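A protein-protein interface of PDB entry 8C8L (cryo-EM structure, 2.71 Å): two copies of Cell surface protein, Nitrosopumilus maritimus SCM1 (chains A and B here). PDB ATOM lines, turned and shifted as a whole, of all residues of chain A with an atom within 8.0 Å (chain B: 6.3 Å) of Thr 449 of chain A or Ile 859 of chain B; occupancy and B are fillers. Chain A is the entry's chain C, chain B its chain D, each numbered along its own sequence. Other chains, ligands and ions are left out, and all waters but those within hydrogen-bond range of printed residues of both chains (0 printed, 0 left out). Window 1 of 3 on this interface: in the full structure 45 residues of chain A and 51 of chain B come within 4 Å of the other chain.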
ATOM      1  N   LEU A 267     -32.552 -12.310  16.264  1.00  0.00           N
ATOM      2  CA  LEU A 267     -32.282 -12.590  14.832  1.00  0.00           C
ATOM      3  C   LEU A 267     -32.497 -14.075  14.565  1.00  0.00           C
ATOM      4  O   LEU A 267     -32.245 -14.916  15.450  1.00  0.00           O
ATOM      5  CB  LEU A 267     -30.852 -12.184  14.475  1.00  0.00           C
ATOM      6  CG  LEU A 267     -30.521 -10.727  14.757  1.00  0.00           C
ATOM      7  CD1 LEU A 267     -29.037 -10.501  14.697  1.00  0.00           C
ATOM      8  CD2 LEU A 267     -31.230  -9.825  13.784  1.00  0.00           C
ATOM      9  N   ARG A 269     -30.834 -16.191  12.597  1.00  0.00           N
ATOM     10  CA  ARG A 269     -29.642 -17.075  12.539  1.00  0.00           C
ATOM     11  C   ARG A 269     -28.455 -16.424  13.240  1.00  0.00           C
ATOM     12  O   ARG A 269     -28.497 -15.213  13.505  1.00  0.00           O
ATOM     13  CB  ARG A 269     -29.214 -17.364  11.101  1.00  0.00           C
ATOM     14  CG  ARG A 269     -30.283 -17.088  10.063  1.00  0.00           C
ATOM     15  CD  ARG A 269     -29.684 -16.785   8.731  1.00  0.00           C
ATOM     16  NE  ARG A 269     -29.161 -17.992   8.157  1.00  0.00           N
ATOM     17  CZ  ARG A 269     -29.438 -18.447   6.941  1.00  0.00           C
ATOM     18  NH1 ARG A 269     -30.256 -17.811   6.125  1.00  0.00           N
ATOM     19  NH2 ARG A 269     -28.841 -19.539   6.541  1.00  0.00           N
ATOM     20  N   THR A 270     -27.390 -17.207  13.409  1.00  0.00           N
ATOM     21  CA  THR A 270     -26.083 -16.759  13.944  1.00  0.00           C
ATOM     22  C   THR A 270     -25.199 -16.263  12.802  1.00  0.00           C
ATOM     23  O   THR A 270     -24.667 -15.134  12.912  1.00  0.00           O
ATOM     24  CB  THR A 270     -25.425 -17.887  14.732  1.00  0.00           C
ATOM     25  OG1 THR A 270     -25.548 -19.093  13.975  1.00  0.00           O
ATOM     26  CG2 THR A 270     -26.074 -18.070  16.084  1.00  0.00           C
ATOM     27  N   VAL A 271     -25.046 -17.063  11.751  1.00  0.00           N
ATOM     28  CA  VAL A 271     -24.124 -16.719  10.639  1.00  0.00           C
ATOM     29  C   VAL A 271     -24.943 -16.524   9.369  1.00  0.00           C
ATOM     30  O   VAL A 271     -25.868 -17.296   9.124  1.00  0.00           O
ATOM     31  CB  VAL A 271     -23.020 -17.771  10.485  1.00  0.00           C
ATOM     32  CG1 VAL A 271     -23.552 -19.108  10.038  1.00  0.00           C
ATOM     33  CG2 VAL A 271     -21.973 -17.279   9.526  1.00  0.00           C
ATOM     34  N   PHE A 272     -24.620 -15.522   8.574  1.00  0.00           N
ATOM     35  CA  PHE A 272     -25.478 -15.148   7.430  1.00  0.00           C
ATOM     36  C   PHE A 272     -24.694 -15.278   6.136  1.00  0.00           C
ATOM     37  O   PHE A 272     -23.688 -14.596   5.960  1.00  0.00           O
ATOM     38  CB  PHE A 272     -25.978 -13.726   7.605  1.00  0.00           C
ATOM     39  CG  PHE A 272     -27.085 -13.564   8.600  1.00  0.00           C
ATOM     40  CD1 PHE A 272     -28.396 -13.565   8.172  1.00  0.00           C
ATOM     41  CD2 PHE A 272     -26.829 -13.330   9.936  1.00  0.00           C
ATOM     42  CE1 PHE A 272     -29.437 -13.375   9.067  1.00  0.00           C
ATOM     43  CE2 PHE A 272     -27.868 -13.145  10.835  1.00  0.00           C
ATOM     44  CZ  PHE A 272     -29.170 -13.171  10.402  1.00  0.00           C
ATOM     45  N   VAL A 278     -32.319 -10.872   6.405  1.00  0.00           N
ATOM     46  CA  VAL A 278     -32.106 -10.671   7.864  1.00  0.00           C
ATOM     47  C   VAL A 278     -33.472 -10.496   8.526  1.00  0.00           C
ATOM     48  O   VAL A 278     -34.049  -9.433   8.432  1.00  0.00           O
ATOM     49  CB  VAL A 278     -31.188  -9.466   8.079  1.00  0.00           C
ATOM     50  CG1 VAL A 278     -30.955  -9.194   9.544  1.00  0.00           C
ATOM     51  CG2 VAL A 278     -29.899  -9.677   7.346  1.00  0.00           C
ATOM     52  N   ALA A 353     -19.436  -2.239  10.016  1.00  0.00           N
ATOM     53  CA  ALA A 353     -18.963  -2.089  11.400  1.00  0.00           C
ATOM     54  C   ALA A 353     -17.447  -1.882  11.401  1.00  0.00           C
ATOM     55  O   ALA A 353     -16.970  -1.027  12.169  1.00  0.00           O
ATOM     56  CB  ALA A 353     -19.404  -3.246  12.229  1.00  0.00           C
ATOM     57  N   GLN A 354     -16.719  -2.576  10.532  1.00  0.00           N
ATOM     58  CA  GLN A 354     -15.237  -2.554  10.528  1.00  0.00           C
ATOM     59  C   GLN A 354     -14.723  -1.528   9.517  1.00  0.00           C
ATOM     60  O   GLN A 354     -13.489  -1.403   9.395  1.00  0.00           O
ATOM     61  CB  GLN A 354     -14.671  -3.943  10.242  1.00  0.00           C
ATOM     62  CG  GLN A 354     -14.910  -4.939  11.366  1.00  0.00           C
ATOM     63  CD  GLN A 354     -16.306  -5.504  11.349  1.00  0.00           C
ATOM     64  OE1 GLN A 354     -16.956  -5.509  10.306  1.00  0.00           O
ATOM     65  NE2 GLN A 354     -16.769  -5.979  12.500  1.00  0.00           N
ATOM     66  N   GLY A 436     -16.271 -12.778   7.232  1.00  0.00           N
ATOM     67  CA  GLY A 436     -15.658 -12.316   8.490  1.00  0.00           C
ATOM     68  C   GLY A 436     -16.113 -10.933   8.884  1.00  0.00           C
ATOM     69  O   GLY A 436     -16.112 -10.636  10.076  1.00  0.00           O
ATOM     70  N   THR A 437     -16.529 -10.105   7.942  1.00  0.00           N
ATOM     71  CA  THR A 437     -17.021  -8.737   8.265  1.00  0.00           C
ATOM     72  C   THR A 437     -18.426  -8.814   8.856  1.00  0.00           C
ATOM     73  O   THR A 437     -19.103  -9.827   8.642  1.00  0.00           O
ATOM     74  CB  THR A 437     -16.913  -7.870   7.024  1.00  0.00           C
ATOM     75  OG1 THR A 437     -17.696  -8.481   5.992  1.00  0.00           O
ATOM     76  CG2 THR A 437     -15.465  -7.726   6.613  1.00  0.00           C
ATOM     77  N   SER A 438     -18.861  -7.770   9.547  1.00  0.00           N
ATOM     78  CA  SER A 438     -20.173  -7.765  10.243  1.00  0.00           C
ATOM     79  C   SER A 438     -20.853  -6.405  10.237  1.00  0.00           C
ATOM     80  O   SER A 438     -20.245  -5.412   9.815  1.00  0.00           O
ATOM     81  CB  SER A 438     -20.015  -8.236  11.632  1.00  0.00           C
ATOM     82  OG  SER A 438     -19.172  -7.367  12.350  1.00  0.00           O
ATOM     83  N   ALA A 439     -22.113  -6.393  10.652  1.00  0.00           N
ATOM     84  CA  ALA A 439     -22.898  -5.163  10.891  1.00  0.00           C
ATOM     85  C   ALA A 439     -23.397  -5.206  12.335  1.00  0.00           C
ATOM     86  O   ALA A 439     -23.128  -6.213  13.045  1.00  0.00           O
ATOM     87  CB  ALA A 439     -24.016  -5.087   9.890  1.00  0.00           C
ATOM     88  N   SER A 440     -24.037  -4.145  12.815  1.00  0.00           N
ATOM     89  CA  SER A 440     -24.501  -4.090  14.219  1.00  0.00           C
ATOM     90  C   SER A 440     -25.889  -3.474  14.269  1.00  0.00           C
ATOM     91  O   SER A 440     -26.024  -2.373  13.777  1.00  0.00           O
ATOM     92  CB  SER A 440     -23.498  -3.365  15.075  1.00  0.00           C
ATOM     93  OG  SER A 440     -23.646  -1.969  14.966  1.00  0.00           O
ATOM     94  N   LEU A 441     -26.878  -4.188  14.803  1.00  0.00           N
ATOM     95  CA  LEU A 441     -28.276  -3.699  14.941  1.00  0.00           C
ATOM     96  C   LEU A 441     -28.589  -3.509  16.424  1.00  0.00           C
ATOM     97  O   LEU A 441     -28.353  -4.448  17.148  1.00  0.00           O
ATOM     98  CB  LEU A 441     -29.194  -4.751  14.323  1.00  0.00           C
ATOM     99  CG  LEU A 441     -30.655  -4.368  14.202  1.00  0.00           C
ATOM    100  CD1 LEU A 441     -30.790  -3.096  13.364  1.00  0.00           C
ATOM    101  CD2 LEU A 441     -31.441  -5.522  13.589  1.00  0.00           C
ATOM    102  N   ASP A 442     -29.167  -2.399  16.872  1.00  0.00           N
ATOM    103  CA  ASP A 442     -29.414  -2.170  18.328  1.00  0.00           C
ATOM    104  C   ASP A 442     -30.873  -1.829  18.692  1.00  0.00           C
ATOM    105  O   ASP A 442     -31.362  -0.781  18.244  1.00  0.00           O
ATOM    106  CB  ASP A 442     -28.562  -1.011  18.830  1.00  0.00           C
ATOM    107  CG  ASP A 442     -28.950  -0.603  20.240  1.00  0.00           C
ATOM    108  OD1 ASP A 442     -28.627  -1.369  21.124  1.00  0.00           O
ATOM    109  OD2 ASP A 442     -29.607   0.456  20.442  1.00  0.00           O
ATOM    110  N   THR A 446     -28.896  -2.785  23.686  1.00  0.00           N
ATOM    111  CA  THR A 446     -28.166  -4.072  23.635  1.00  0.00           C
ATOM    112  C   THR A 446     -27.856  -4.379  22.183  1.00  0.00           C
ATOM    113  O   THR A 446     -28.740  -4.850  21.480  1.00  0.00           O
ATOM    114  CB  THR A 446     -29.045  -5.238  24.095  1.00  0.00           C
ATOM    115  OG1 THR A 446     -29.804  -4.794  25.213  1.00  0.00           O
ATOM    116  CG2 THR A 446     -28.230  -6.469  24.411  1.00  0.00           C
ATOM    117  N   PRO A 447     -26.663  -4.090  21.650  1.00  0.00           N
ATOM    118  CA  PRO A 447     -26.415  -4.345  20.231  1.00  0.00           C
ATOM    119  C   PRO A 447     -26.151  -5.814  19.905  1.00  0.00           C
ATOM    120  O   PRO A 447     -25.744  -6.545  20.791  1.00  0.00           O
ATOM    121  CB  PRO A 447     -25.227  -3.435  19.928  1.00  0.00           C
ATOM    122  CG  PRO A 447     -24.497  -3.385  21.224  1.00  0.00           C
ATOM    123  CD  PRO A 447     -25.557  -3.391  22.305  1.00  0.00           C
ATOM    124  N   GLN A 448     -26.439  -6.220  18.669  1.00  0.00           N
ATOM    125  CA  GLN A 448     -26.200  -7.597  18.167  1.00  0.00           C
ATOM    126  C   GLN A 448     -25.425  -7.504  16.857  1.00  0.00           C
ATOM    127  O   GLN A 448     -25.783  -6.670  16.023  1.00  0.00           O
ATOM    128  CB  GLN A 448     -27.526  -8.328  18.006  1.00  0.00           C
ATOM    129  CG  GLN A 448     -28.136  -8.645  19.352  1.00  0.00           C
ATOM    130  CD  GLN A 448     -29.222  -9.682  19.280  1.00  0.00           C
ATOM    131  OE1 GLN A 448     -30.216  -9.509  18.600  1.00  0.00           O
ATOM    132  NE2 GLN A 448     -29.048 -10.773  20.007  1.00  0.00           N
ATOM    133  N   THR A 449     -24.415  -8.337  16.684  1.00  0.00           N
ATOM    134  CA  THR A 449     -23.647  -8.395  15.420  1.00  0.00           C
ATOM    135  C   THR A 449     -24.386  -9.250  14.383  1.00  0.00           C
ATOM    136  O   THR A 449     -25.024 -10.231  14.743  1.00  0.00           O
ATOM    137  CB  THR A 449     -22.217  -8.892  15.637  1.00  0.00           C
ATOM    138  OG1 THR A 449     -21.602  -8.920  14.353  1.00  0.00           O
ATOM    139  CG2 THR A 449     -22.136 -10.271  16.244  1.00  0.00           C
ATOM    140  N   ILE A 450     -24.262  -8.878  13.121  1.00  0.00           N
ATOM    141  CA  ILE A 450     -24.762  -9.677  11.973  1.00  0.00           C
ATOM    142  C   ILE A 450     -23.527 -10.139  11.214  1.00  0.00           C
ATOM    143  O   ILE A 450     -23.002  -9.396  10.386  1.00  0.00           O
ATOM    144  CB  ILE A 450     -25.699  -8.814  11.123  1.00  0.00           C
ATOM    145  CG1 ILE A 450     -26.901  -8.351  11.948  1.00  0.00           C
ATOM    146  CG2 ILE A 450     -26.091  -9.529   9.844  1.00  0.00           C
ATOM    147  CD1 ILE A 450     -27.615  -7.176  11.361  1.00  0.00           C
ATOM    148  N   LEU A 451     -23.046 -11.314  11.545  1.00  0.00           N
ATOM    149  CA  LEU A 451     -21.766 -11.820  11.010  1.00  0.00           C
ATOM    150  C   LEU A 451     -22.016 -12.524   9.674  1.00  0.00           C
ATOM    151  O   LEU A 451     -22.988 -13.297   9.543  1.00  0.00           O
ATOM    152  CB  LEU A 451     -21.199 -12.776  12.048  1.00  0.00           C
ATOM    153  CG  LEU A 451     -19.819 -13.339  11.761  1.00  0.00           C
ATOM    154  CD1 LEU A 451     -18.717 -12.280  11.880  1.00  0.00           C
ATOM    155  CD2 LEU A 451     -19.560 -14.459  12.742  1.00  0.00           C
ATOM    156  N   VAL A 452     -21.134 -12.296   8.721  1.00  0.00           N
ATOM    157  CA  VAL A 452     -21.179 -12.988   7.407  1.00  0.00           C
ATOM    158  C   VAL A 452     -20.158 -14.123   7.392  1.00  0.00           C
ATOM    159  O   VAL A 452     -18.999 -13.864   7.692  1.00  0.00           O
ATOM    160  CB  VAL A 452     -20.941 -11.990   6.278  1.00  0.00           C
ATOM    161  CG1 VAL A 452     -20.550 -12.689   4.997  1.00  0.00           C
ATOM    162  CG2 VAL A 452     -22.188 -11.166   6.087  1.00  0.00           C
ATOM    163  N   ASP B 855     -15.479  -4.529  23.435  1.00  0.00           N
ATOM    164  CA  ASP B 855     -16.943  -4.397  23.666  1.00  0.00           C
ATOM    165  C   ASP B 855     -17.497  -5.745  24.105  1.00  0.00           C
ATOM    166  O   ASP B 855     -17.155  -6.767  23.485  1.00  0.00           O
ATOM    167  CB  ASP B 855     -17.657  -3.883  22.421  1.00  0.00           C
ATOM    168  CG  ASP B 855     -19.091  -3.427  22.645  1.00  0.00           C
ATOM    169  OD1 ASP B 855     -19.736  -3.927  23.589  1.00  0.00           O
ATOM    170  OD2 ASP B 855     -19.527  -2.504  21.920  1.00  0.00           O
ATOM    171  N   ASP B 857     -20.840  -6.467  24.179  1.00  0.00           N
ATOM    172  CA  ASP B 857     -22.106  -6.756  23.459  1.00  0.00           C
ATOM    173  C   ASP B 857     -21.819  -7.263  22.041  1.00  0.00           C
ATOM    174  O   ASP B 857     -22.635  -8.028  21.511  1.00  0.00           O
ATOM    175  CB  ASP B 857     -22.974  -5.508  23.418  1.00  0.00           C
ATOM    176  CG  ASP B 857     -23.100  -4.854  24.779  1.00  0.00           C
ATOM    177  OD1 ASP B 857     -23.615  -5.521  25.708  1.00  0.00           O
ATOM    178  OD2 ASP B 857     -22.645  -3.693  24.909  1.00  0.00           O
ATOM    179  N   LEU B 858     -20.719  -6.840  21.424  1.00  0.00           N
ATOM    180  CA  LEU B 858     -20.524  -7.041  19.959  1.00  0.00           C
ATOM    181  C   LEU B 858     -19.378  -7.995  19.716  1.00  0.00           C
ATOM    182  O   LEU B 858     -18.575  -7.897  20.431  1.00  0.00           O
ATOM    183  CB  LEU B 858     -20.126  -5.710  19.350  1.00  0.00           C
ATOM    184  CG  LEU B 858     -21.275  -4.769  19.103  1.00  0.00           C
ATOM    185  CD1 LEU B 858     -20.776  -3.575  18.315  1.00  0.00           C
ATOM    186  CD2 LEU B 858     -22.389  -5.474  18.358  1.00  0.00           C
ATOM    187  N   ILE B 859     -19.298  -8.732  18.616  1.00  0.00           N
ATOM    188  CA  ILE B 859     -18.103  -9.556  18.295  1.00  0.00           C
ATOM    189  C   ILE B 859     -16.983  -8.647  17.782  1.00  0.00           C
ATOM    190  O   ILE B 859     -17.255  -7.815  16.912  1.00  0.00           O
ATOM    191  CB  ILE B 859     -18.505 -10.662  17.307  1.00  0.00           C
ATOM    192  CG1 ILE B 859     -19.179 -11.787  18.097  1.00  0.00           C
ATOM    193  CG2 ILE B 859     -17.322 -11.150  16.479  1.00  0.00           C
ATOM    194  CD1 ILE B 859     -19.684 -12.904  17.251  1.00  0.00           C
ATOM    195  N   ASP B 860     -15.769  -8.798  18.293  1.00  0.00           N
ATOM    196  CA  ASP B 860     -14.646  -7.914  17.878  1.00  0.00           C
ATOM    197  C   ASP B 860     -13.874  -8.510  16.689  1.00  0.00           C
ATOM    198  O   ASP B 860     -13.429  -9.672  16.768  1.00  0.00           O
ATOM    199  CB  ASP B 860     -13.730  -7.643  19.062  1.00  0.00           C
ATOM    200  CG  ASP B 860     -14.389  -6.926  20.235  1.00  0.00           C
ATOM    201  OD1 ASP B 860     -15.439  -6.281  20.111  1.00  0.00           O
ATOM    202  OD2 ASP B 860     -13.866  -7.085  21.317  1.00  0.00           O
ATOM    203  N   ILE B 861     -13.678  -7.723  15.628  1.00  0.00           N
ATOM    204  CA  ILE B 861     -13.076  -8.192  14.341  1.00  0.00           C
ATOM    205  C   ILE B 861     -11.898  -7.313  13.928  1.00  0.00           C
ATOM    206  O   ILE B 861     -11.941  -6.098  14.119  1.00  0.00           O
ATOM    207  CB  ILE B 861     -14.143  -8.247  13.248  1.00  0.00           C
ATOM    208  CG1 ILE B 861     -15.317  -9.117  13.724  1.00  0.00           C
ATOM    209  CG2 ILE B 861     -13.522  -8.713  11.948  1.00  0.00           C
ATOM    210  CD1 ILE B 861     -16.437  -9.256  12.747  1.00  0.00           C
ATOM    211  N   VAL B 942     -11.652 -13.064  14.001  1.00  0.00           N
ATOM    212  CA  VAL B 942     -13.039 -12.950  14.521  1.00  0.00           C
ATOM    213  C   VAL B 942     -13.087 -13.496  15.941  1.00  0.00           C
ATOM    214  O   VAL B 942     -12.609 -14.612  16.181  1.00  0.00           O
ATOM    215  CB  VAL B 942     -13.988 -13.695  13.598  1.00  0.00           C
ATOM    216  CG1 VAL B 942     -15.420 -13.613  14.081  1.00  0.00           C
ATOM    217  CG2 VAL B 942     -13.820 -13.162  12.184  1.00  0.00           C
ATOM    218  N   GLU B 943     -13.636 -12.723  16.859  1.00  0.00           N
ATOM    219  CA  GLU B 943     -13.806 -13.159  18.257  1.00  0.00           C
ATOM    220  C   GLU B 943     -14.870 -14.256  18.296  1.00  0.00           C
ATOM    221  O   GLU B 943     -15.955 -14.062  17.725  1.00  0.00           O
ATOM    222  CB  GLU B 943     -14.244 -11.997  19.122  1.00  0.00           C
ATOM    223  CG  GLU B 943     -14.205 -12.314  20.604  1.00  0.00           C
ATOM    224  CD  GLU B 943     -14.540 -11.100  21.474  1.00  0.00           C
ATOM    225  OE1 GLU B 943     -14.813 -10.053  20.875  1.00  0.00           O
ATOM    226  OE2 GLU B 943     -14.558 -11.225  22.726  1.00  0.00           O
ATOM    227  N   THR B 944     -14.578 -15.342  18.988  1.00  0.00           N
ATOM    228  CA  THR B 944     -15.454 -16.538  19.082  1.00  0.00           C
ATOM    229  C   THR B 944     -16.793 -16.154  19.722  1.00  0.00           C
ATOM    230  O   THR B 944     -17.823 -16.554  19.173  1.00  0.00           O
ATOM    231  CB  THR B 944     -14.762 -17.658  19.857  1.00  0.00           C
ATOM    232  OG1 THR B 944     -14.358 -17.146  21.122  1.00  0.00           O
ATOM    233  CG2 THR B 944     -13.534 -18.179  19.152  1.00  0.00           C
ATOM    234  N   GLY B 945     -16.772 -15.361  20.801  1.00  0.00           N
ATOM    235  CA  GLY B 945     -17.985 -14.890  21.496  1.00  0.00           C
ATOM    236  C   GLY B 945     -18.047 -13.380  21.580  1.00  0.00           C
ATOM    237  O   GLY B 945     -17.208 -12.705  21.017  1.00  0.00           O
ATOM    238  N   ALA B 946     -19.024 -12.842  22.291  1.00  0.00           N
ATOM    239  CA  ALA B 946     -19.199 -11.382  22.405  1.00  0.00           C
ATOM    240  C   ALA B 946     -18.087 -10.815  23.288  1.00  0.00           C
ATOM    241  O   ALA B 946     -17.557  -9.714  22.944  1.00  0.00           O
ATOM    242  CB  ALA B 946     -20.547 -11.086  22.975  1.00  0.00           C
ATOM    243  N   PHE B 951      -9.747 -14.971  19.440  1.00  0.00           N
ATOM    244  CA  PHE B 951      -9.895 -14.572  18.029  1.00  0.00           C
ATOM    245  C   PHE B 951      -9.389 -15.695  17.143  1.00  0.00           C
ATOM    246  O   PHE B 951      -8.347 -16.257  17.426  1.00  0.00           O
ATOM    247  CB  PHE B 951      -9.129 -13.279  17.781  1.00  0.00           C
ATOM    248  CG  PHE B 951      -9.678 -12.131  18.580  1.00  0.00           C
ATOM    249  CD1 PHE B 951      -9.330 -11.993  19.905  1.00  0.00           C
ATOM    250  CD2 PHE B 951     -10.598 -11.237  18.033  1.00  0.00           C
ATOM    251  CE1 PHE B 951      -9.851 -10.957  20.666  1.00  0.00           C
ATOM    252  CE2 PHE B 951     -11.119 -10.199  18.797  1.00  0.00           C
ATOM    253  CZ  PHE B 951     -10.752 -10.069  20.117  1.00  0.00           C
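OG of Ser 438 of chain A sits at hydrogen-bond distance from NE2 of Gln 354 of chain A, 2.8 Å away. The backbone NH of Gly 436 of chain A sits at hydrogen-bond distance from the backbone carbonyl oxygen of Val 452 of chain A, at 3.0 Å. The backbone NH of Ala 353 of chain A is in hydrogen-bond range of the backbone carbonyl oxygen of Ser 438 of chain A (3.3 Å). OD1 of Asp 855 of chain B is in hydrogen-bond range of N of Asp 857 of chain B, 2.8 Å away. O of Leu 451 of chain A sits at hydrogen-bond distance from N of Phe 272 of chain A, at 2.9 Å. O of Ala 439 of chain A sits close to OG1 of Thr 449 of chain A, 3.4 Å away.
Among the printed residues, pairs that only touch across the chains: Gly 436 of chain A with Ile 861 of chain B (3.0 Å), Gln 354 of chain A with Ile 861 of chain B (3.3 Å), Ser 438 of chain A with Ile 861 of chain B (3.3 Å), Pro 447 of chain A with Asp 857 of chain B (3.4 Å), Thr 449 of chain A with Ile 859 of chain B (3.7 Å), Pro 447 of chain A with Leu 858 of chain B (3.8 Å), Leu 451 of chain A with Ile 861 of chain B (3.9 Å), Thr 449 of chain A with Leu 858 of chain B (3.9 Å) and Gln 448 of chain A with Leu 858 of chain B (3.9 Å).
Thr 449 of chain A touches just these residues of chain B: Leu 858 (3.9 Å) and Ile 859 (3.7 Å). Printed residues of chain A within 4 Å of Ile 859 of chain B: Thr 449. Of the printed residues of chain B, Gly 436 of chain A touches Ile 861 (3.0 Å). Printed residues of chain B within 4 Å of Leu 451 of chain A: Ile 861 (3.9 Å). Of the printed residues of chain B, Ser 438 of chain A touches Ile 861 (3.3 Å). Asp 860 of chain B touches none of the printed residues of chain A. Thr 446 of chain A touches none of the printed residues of chain B. The nearest residue of chain B that does not touch Thr 449 of chain A is Asp 857 of chain B (5.2 Å).
Of the 12 printed residues of chain B, 4 touch a printed residue of chain A. Printed residues of chain B that touch a printed residue of chain A: Asp 857, Leu 858, Ile 859 and Ile 861. Hydrophobic or aromatic side chains of chain B within 4 Å of the printed part of chain A: Leu 858, Ile 859 and Ile 861. Of the 22 printed residues of chain A, 7 touch a printed residue of chain B. Printed residues of chain A that touch a printed residue of chain B: Gln 354, Gly 436, Ser 438, Pro 447, Gln 448, Thr 449 and Leu 451. Hydrophobic or aromatic side chains of chain A that line the printed part of chain B: Pro 447 and Leu 451. Among the printed residues, no Asp or Glu carboxylate lies within 4 Å of a Lys or Arg side-chain nitrogen of the other chain.
No position is printed for both chains.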
